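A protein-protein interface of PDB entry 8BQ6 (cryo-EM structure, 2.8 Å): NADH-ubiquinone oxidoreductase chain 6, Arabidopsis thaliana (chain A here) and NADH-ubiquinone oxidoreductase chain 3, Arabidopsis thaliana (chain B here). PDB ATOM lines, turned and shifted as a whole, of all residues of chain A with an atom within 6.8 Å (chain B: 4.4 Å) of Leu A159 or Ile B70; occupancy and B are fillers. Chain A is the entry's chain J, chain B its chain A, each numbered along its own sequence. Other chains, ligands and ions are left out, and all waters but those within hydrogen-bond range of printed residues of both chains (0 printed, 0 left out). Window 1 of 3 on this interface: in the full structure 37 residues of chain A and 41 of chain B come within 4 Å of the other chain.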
ATOM      1  N   ALA A  60     -18.056   6.242  37.059  1.00  0.00           N
ATOM      2  CA  ALA A  60     -17.342   6.350  35.793  1.00  0.00           C
ATOM      3  C   ALA A  60     -18.031   7.246  34.777  1.00  0.00           C
ATOM      4  O   ALA A  60     -17.370   8.081  34.152  1.00  0.00           O
ATOM      5  CB  ALA A  60     -17.133   4.950  35.199  1.00  0.00           C
ATOM      6  N   VAL A 154     -19.729  -9.635  21.894  1.00  0.00           N
ATOM      7  CA  VAL A 154     -20.184  -8.510  21.076  1.00  0.00           C
ATOM      8  C   VAL A 154     -20.117  -7.212  21.876  1.00  0.00           C
ATOM      9  O   VAL A 154     -19.783  -6.145  21.340  1.00  0.00           O
ATOM     10  CB  VAL A 154     -21.602  -8.773  20.535  1.00  0.00           C
ATOM     11  CG1 VAL A 154     -22.144  -7.537  19.844  1.00  0.00           C
ATOM     12  CG2 VAL A 154     -21.597  -9.944  19.572  1.00  0.00           C
ATOM     13  N   SER A 155     -20.434  -7.280  23.171  1.00  0.00           N
ATOM     14  CA  SER A 155     -20.296  -6.099  24.018  1.00  0.00           C
ATOM     15  C   SER A 155     -18.838  -5.661  24.120  1.00  0.00           C
ATOM     16  O   SER A 155     -18.540  -4.458  24.151  1.00  0.00           O
ATOM     17  CB  SER A 155     -20.892  -6.372  25.401  1.00  0.00           C
ATOM     18  OG  SER A 155     -19.963  -7.001  26.264  1.00  0.00           O
ATOM     19  N   SER A 156     -17.912  -6.622  24.173  1.00  0.00           N
ATOM     20  CA  SER A 156     -16.496  -6.250  24.105  1.00  0.00           C
ATOM     21  C   SER A 156     -16.172  -5.513  22.806  1.00  0.00           C
ATOM     22  O   SER A 156     -15.389  -4.555  22.802  1.00  0.00           O
ATOM     23  CB  SER A 156     -15.609  -7.483  24.248  1.00  0.00           C
ATOM     24  OG  SER A 156     -15.438  -8.144  23.010  1.00  0.00           O
ATOM     25  N   LEU A 157     -16.747  -5.961  21.688  1.00  0.00           N
ATOM     26  CA  LEU A 157     -16.517  -5.265  20.421  1.00  0.00           C
ATOM     27  C   LEU A 157     -17.044  -3.832  20.475  1.00  0.00           C
ATOM     28  O   LEU A 157     -16.421  -2.901  19.943  1.00  0.00           O
ATOM     29  CB  LEU A 157     -17.168  -6.036  19.276  1.00  0.00           C
ATOM     30  CG  LEU A 157     -16.405  -7.281  18.832  1.00  0.00           C
ATOM     31  CD1 LEU A 157     -17.092  -7.910  17.641  1.00  0.00           C
ATOM     32  CD2 LEU A 157     -14.967  -6.933  18.500  1.00  0.00           C
ATOM     33  N   ILE A 158     -18.195  -3.644  21.123  1.00  0.00           N
ATOM     34  CA  ILE A 158     -18.752  -2.306  21.322  1.00  0.00           C
ATOM     35  C   ILE A 158     -17.786  -1.426  22.122  1.00  0.00           C
ATOM     36  O   ILE A 158     -17.542  -0.256  21.777  1.00  0.00           O
ATOM     37  CB  ILE A 158     -20.134  -2.429  21.995  1.00  0.00           C
ATOM     38  CG1 ILE A 158     -21.203  -2.774  20.954  1.00  0.00           C
ATOM     39  CG2 ILE A 158     -20.496  -1.180  22.760  1.00  0.00           C
ATOM     40  CD1 ILE A 158     -22.453  -3.387  21.537  1.00  0.00           C
ATOM     41  N   LEU A 159     -17.208  -1.976  23.191  1.00  0.00           N
ATOM     42  CA  LEU A 159     -16.248  -1.203  23.980  1.00  0.00           C
ATOM     43  C   LEU A 159     -14.999  -0.857  23.169  1.00  0.00           C
ATOM     44  O   LEU A 159     -14.469   0.261  23.271  1.00  0.00           O
ATOM     45  CB  LEU A 159     -15.873  -1.964  25.250  1.00  0.00           C
ATOM     46  CG  LEU A 159     -16.989  -2.090  26.287  1.00  0.00           C
ATOM     47  CD1 LEU A 159     -16.528  -2.942  27.450  1.00  0.00           C
ATOM     48  CD2 LEU A 159     -17.426  -0.717  26.763  1.00  0.00           C
ATOM     49  N   LEU A 160     -14.509  -1.808  22.367  1.00  0.00           N
ATOM     50  CA  LEU A 160     -13.367  -1.535  21.494  1.00  0.00           C
ATOM     51  C   LEU A 160     -13.660  -0.377  20.550  1.00  0.00           C
ATOM     52  O   LEU A 160     -12.802   0.494  20.334  1.00  0.00           O
ATOM     53  CB  LEU A 160     -13.001  -2.787  20.696  1.00  0.00           C
ATOM     54  CG  LEU A 160     -11.851  -2.691  19.683  1.00  0.00           C
ATOM     55  CD1 LEU A 160     -10.587  -2.139  20.304  1.00  0.00           C
ATOM     56  CD2 LEU A 160     -11.582  -4.025  19.017  1.00  0.00           C
ATOM     57  N   VAL A 161     -14.861  -0.356  19.966  1.00  0.00           N
ATOM     58  CA  VAL A 161     -15.226   0.753  19.090  1.00  0.00           C
ATOM     59  C   VAL A 161     -15.198   2.068  19.857  1.00  0.00           C
ATOM     60  O   VAL A 161     -14.750   3.096  19.336  1.00  0.00           O
ATOM     61  CB  VAL A 161     -16.597   0.508  18.435  1.00  0.00           C
ATOM     62  CG1 VAL A 161     -17.072   1.761  17.710  1.00  0.00           C
ATOM     63  CG2 VAL A 161     -16.509  -0.651  17.469  1.00  0.00           C
ATOM     64  N   ALA A 162     -15.680   2.065  21.103  1.00  0.00           N
ATOM     65  CA  ALA A 162     -15.648   3.302  21.882  1.00  0.00           C
ATOM     66  C   ALA A 162     -14.214   3.796  22.090  1.00  0.00           C
ATOM     67  O   ALA A 162     -13.934   4.991  21.941  1.00  0.00           O
ATOM     68  CB  ALA A 162     -16.359   3.110  23.221  1.00  0.00           C
ATOM     69  N   MET A 163     -13.288   2.888  22.417  1.00  0.00           N
ATOM     70  CA  MET A 163     -11.894   3.300  22.627  1.00  0.00           C
ATOM     71  C   MET A 163     -11.278   3.861  21.347  1.00  0.00           C
ATOM     72  O   MET A 163     -10.632   4.926  21.354  1.00  0.00           O
ATOM     73  CB  MET A 163     -11.062   2.125  23.148  1.00  0.00           C
ATOM     74  CG  MET A 163     -11.762   1.321  24.221  1.00  0.00           C
ATOM     75  SD  MET A 163     -11.031  -0.271  24.656  1.00  0.00           S
ATOM     76  CE  MET A 163      -9.421   0.222  25.236  1.00  0.00           C
ATOM     77  N   ILE A 164     -11.484   3.160  20.230  1.00  0.00           N
ATOM     78  CA  ILE A 164     -10.927   3.608  18.958  1.00  0.00           C
ATOM     79  C   ILE A 164     -11.483   4.975  18.591  1.00  0.00           C
ATOM     80  O   ILE A 164     -10.734   5.899  18.257  1.00  0.00           O
ATOM     81  CB  ILE A 164     -11.215   2.575  17.855  1.00  0.00           C
ATOM     82  CG1 ILE A 164     -10.183   1.455  17.896  1.00  0.00           C
ATOM     83  CG2 ILE A 164     -11.205   3.240  16.487  1.00  0.00           C
ATOM     84  CD1 ILE A 164     -10.550   0.279  17.034  1.00  0.00           C
ATOM     85  N   ILE B  66     -12.184   8.196  29.655  1.00  0.00           N
ATOM     86  CA  ILE B  66     -12.588   7.096  28.775  1.00  0.00           C
ATOM     87  C   ILE B  66     -11.896   5.804  29.181  1.00  0.00           C
ATOM     88  O   ILE B  66     -12.515   4.731  29.242  1.00  0.00           O
ATOM     89  CB  ILE B  66     -12.285   7.438  27.307  1.00  0.00           C
ATOM     90  CG1 ILE B  66     -13.119   8.623  26.861  1.00  0.00           C
ATOM     91  CG2 ILE B  66     -12.574   6.249  26.417  1.00  0.00           C
ATOM     92  CD1 ILE B  66     -14.528   8.539  27.310  1.00  0.00           C
ATOM     93  N   LEU B  67     -10.586   5.886  29.421  1.00  0.00           N
ATOM     94  CA  LEU B  67      -9.835   4.703  29.828  1.00  0.00           C
ATOM     95  C   LEU B  67     -10.379   4.127  31.122  1.00  0.00           C
ATOM     96  O   LEU B  67     -10.548   2.902  31.258  1.00  0.00           O
ATOM     97  CB  LEU B  67      -8.371   5.068  29.999  1.00  0.00           C
ATOM     98  CG  LEU B  67      -7.637   5.035  28.679  1.00  0.00           C
ATOM     99  CD1 LEU B  67      -6.376   5.841  28.797  1.00  0.00           C
ATOM    100  CD2 LEU B  67      -7.340   3.592  28.375  1.00  0.00           C
ATOM    101  N   PHE B  68     -10.652   5.001  32.086  1.00  0.00           N
ATOM    102  CA  PHE B  68     -11.189   4.541  33.352  1.00  0.00           C
ATOM    103  C   PHE B  68     -12.536   3.872  33.161  1.00  0.00           C
ATOM    104  O   PHE B  68     -12.813   2.849  33.784  1.00  0.00           O
ATOM    105  CB  PHE B  68     -11.322   5.695  34.329  1.00  0.00           C
ATOM    106  CG  PHE B  68     -12.037   5.316  35.567  1.00  0.00           C
ATOM    107  CD1 PHE B  68     -11.553   4.299  36.358  1.00  0.00           C
ATOM    108  CD2 PHE B  68     -13.205   5.944  35.930  1.00  0.00           C
ATOM    109  CE1 PHE B  68     -12.207   3.929  37.496  1.00  0.00           C
ATOM    110  CE2 PHE B  68     -13.858   5.577  37.070  1.00  0.00           C
ATOM    111  CZ  PHE B  68     -13.361   4.567  37.852  1.00  0.00           C
ATOM    112  N   LEU B  69     -13.393   4.451  32.323  1.00  0.00           N
ATOM    113  CA  LEU B  69     -14.704   3.864  32.082  1.00  0.00           C
ATOM    114  C   LEU B  69     -14.580   2.461  31.500  1.00  0.00           C
ATOM    115  O   LEU B  69     -15.256   1.521  31.948  1.00  0.00           O
ATOM    116  CB  LEU B  69     -15.492   4.772  31.147  1.00  0.00           C
ATOM    117  CG  LEU B  69     -16.779   4.227  30.549  1.00  0.00           C
ATOM    118  CD1 LEU B  69     -17.778   3.868  31.632  1.00  0.00           C
ATOM    119  CD2 LEU B  69     -17.330   5.276  29.624  1.00  0.00           C
ATOM    120  N   ILE B  70     -13.698   2.298  30.510  1.00  0.00           N
ATOM    121  CA  ILE B  70     -13.522   0.985  29.893  1.00  0.00           C
ATOM    122  C   ILE B  70     -13.075  -0.036  30.936  1.00  0.00           C
ATOM    123  O   ILE B  70     -13.639  -1.133  31.046  1.00  0.00           O
ATOM    124  CB  ILE B  70     -12.529   1.065  28.718  1.00  0.00           C
ATOM    125  CG1 ILE B  70     -13.028   2.020  27.626  1.00  0.00           C
ATOM    126  CG2 ILE B  70     -12.287  -0.312  28.132  1.00  0.00           C
ATOM    127  CD1 ILE B  70     -14.469   1.851  27.239  1.00  0.00           C
ATOM    128  N   PHE B  71     -12.074   0.319  31.747  1.00  0.00           N
ATOM    129  CA  PHE B  71     -11.567  -0.672  32.697  1.00  0.00           C
ATOM    130  C   PHE B  71     -12.467  -0.846  33.912  1.00  0.00           C
ATOM    131  O   PHE B  71     -12.423  -1.895  34.564  1.00  0.00           O
ATOM    132  CB  PHE B  71     -10.152  -0.308  33.104  1.00  0.00           C
ATOM    133  CG  PHE B  71      -9.159  -0.668  32.068  1.00  0.00           C
ATOM    134  CD1 PHE B  71      -8.817   0.238  31.083  1.00  0.00           C
ATOM    135  CD2 PHE B  71      -8.618  -1.935  32.030  1.00  0.00           C
ATOM    136  CE1 PHE B  71      -7.920  -0.102  30.103  1.00  0.00           C
ATOM    137  CE2 PHE B  71      -7.723  -2.279  31.053  1.00  0.00           C
ATOM    138  CZ  PHE B  71      -7.371  -1.360  30.089  1.00  0.00           C
ATOM    139  N   ASP B  72     -13.289   0.155  34.210  1.00  0.00           N
ATOM    140  CA  ASP B  72     -14.370   0.019  35.171  1.00  0.00           C
ATOM    141  C   ASP B  72     -15.336  -1.071  34.736  1.00  0.00           C
ATOM    142  O   ASP B  72     -15.733  -1.933  35.533  1.00  0.00           O
ATOM    143  CB  ASP B  72     -15.084   1.365  35.275  1.00  0.00           C
ATOM    144  CG  ASP B  72     -15.801   1.552  36.573  1.00  0.00           C
ATOM    145  OD1 ASP B  72     -17.047   1.594  36.552  1.00  0.00           O
ATOM    146  OD2 ASP B  72     -15.120   1.683  37.607  1.00  0.00           O
ATOM    147  N   LEU B  73     -15.722  -1.047  33.460  1.00  0.00           N
ATOM    148  CA  LEU B  73     -16.561  -2.118  32.937  1.00  0.00           C
ATOM    149  C   LEU B  73     -15.831  -3.456  32.939  1.00  0.00           C
ATOM    150  O   LEU B  73     -16.461  -4.504  33.130  1.00  0.00           O
ATOM    151  CB  LEU B  73     -17.044  -1.771  31.535  1.00  0.00           C
ATOM    152  CG  LEU B  73     -18.199  -0.774  31.538  1.00  0.00           C
ATOM    153  CD1 LEU B  73     -18.333  -0.132  30.181  1.00  0.00           C
ATOM    154  CD2 LEU B  73     -19.495  -1.448  31.962  1.00  0.00           C
ATOM    155  N   GLU B  74     -14.511  -3.453  32.786  1.00  0.00           N
ATOM    156  CA  GLU B  74     -13.748  -4.729  32.841  1.00  0.00           C
ATOM    157  C   GLU B  74     -13.794  -5.309  34.261  1.00  0.00           C
ATOM    158  O   GLU B  74     -14.054  -6.509  34.390  1.00  0.00           O
ATOM    159  CB  GLU B  74     -12.326  -4.518  32.327  1.00  0.00           C
ATOM    160  CG  GLU B  74     -11.515  -5.790  32.226  1.00  0.00           C
ATOM    161  CD  GLU B  74     -10.200  -5.607  31.490  1.00  0.00           C
ATOM    162  OE1 GLU B  74     -10.239  -5.291  30.285  1.00  0.00           O
ATOM    163  OE2 GLU B  74      -9.145  -5.762  32.128  1.00  0.00           O
ATOM    164  N   LEU B 103     -10.228  -6.331  24.613  1.00  0.00           N
ATOM    165  CA  LEU B 103     -10.025  -5.066  25.315  1.00  0.00           C
ATOM    166  C   LEU B 103      -8.542  -4.702  25.425  1.00  0.00           C
ATOM    167  O   LEU B 103      -8.189  -3.517  25.419  1.00  0.00           O
ATOM    168  CB  LEU B 103     -10.703  -5.122  26.684  1.00  0.00           C
ATOM    169  CG  LEU B 103     -12.237  -5.074  26.578  1.00  0.00           C
ATOM    170  CD1 LEU B 103     -12.884  -4.581  27.843  1.00  0.00           C
ATOM    171  CD2 LEU B 103     -12.689  -4.207  25.411  1.00  0.00           C
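Among the printed residues, pairs that only touch across the chains: Leu A159 with Leu B73, Ala A60 with Asp B72, Met A163 with Ile B70, Ser A156 with Leu B103, Ala A60 with Leu B69, Ala A60 with Phe B68, Leu A159 with Leu B103, Met A163 with Leu B103 and Leu A159 with Ile B70.
Of chain B, only Ile B70 (3.9 Å), Leu B73 (3.6 Å) and Leu B103 (3.9 Å) come within 4 Å of Leu A159. Ile B70 touches just these residues of chain A: Leu A159 and Met A163. Of the printed residues of chain B, Met A163 touches Ile B70 and Leu B103. Of the printed residues of chain A, Asp B72 touches Ala A60. Printed residues of chain B within 4 Å of Ala A60: Phe B68 (3.8 Å), Leu B69 (3.8 Å) and Asp B72 (3.6 Å). Printed residues of chain A within 4 Å of Leu B69: Ala A60. Printed residues of chain A within 4 Å of Leu B73: Leu A159 (3.6 Å). The nearest printed residue of chain A that does not touch Phe B68 is Met A163 (8.4 Å).
Of the 10 printed residues of chain B, 6 touch a printed residue of chain A. Hydrophobic or aromatic side chains of chain B that line the printed part of chain A: Phe B68, Leu B69, Ile B70, Leu B73 and Leu B103. Hydrophobic or aromatic side chains of chain A within 4 Å of the printed part of chain B: Ala A60, Leu A159 and Met A163.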
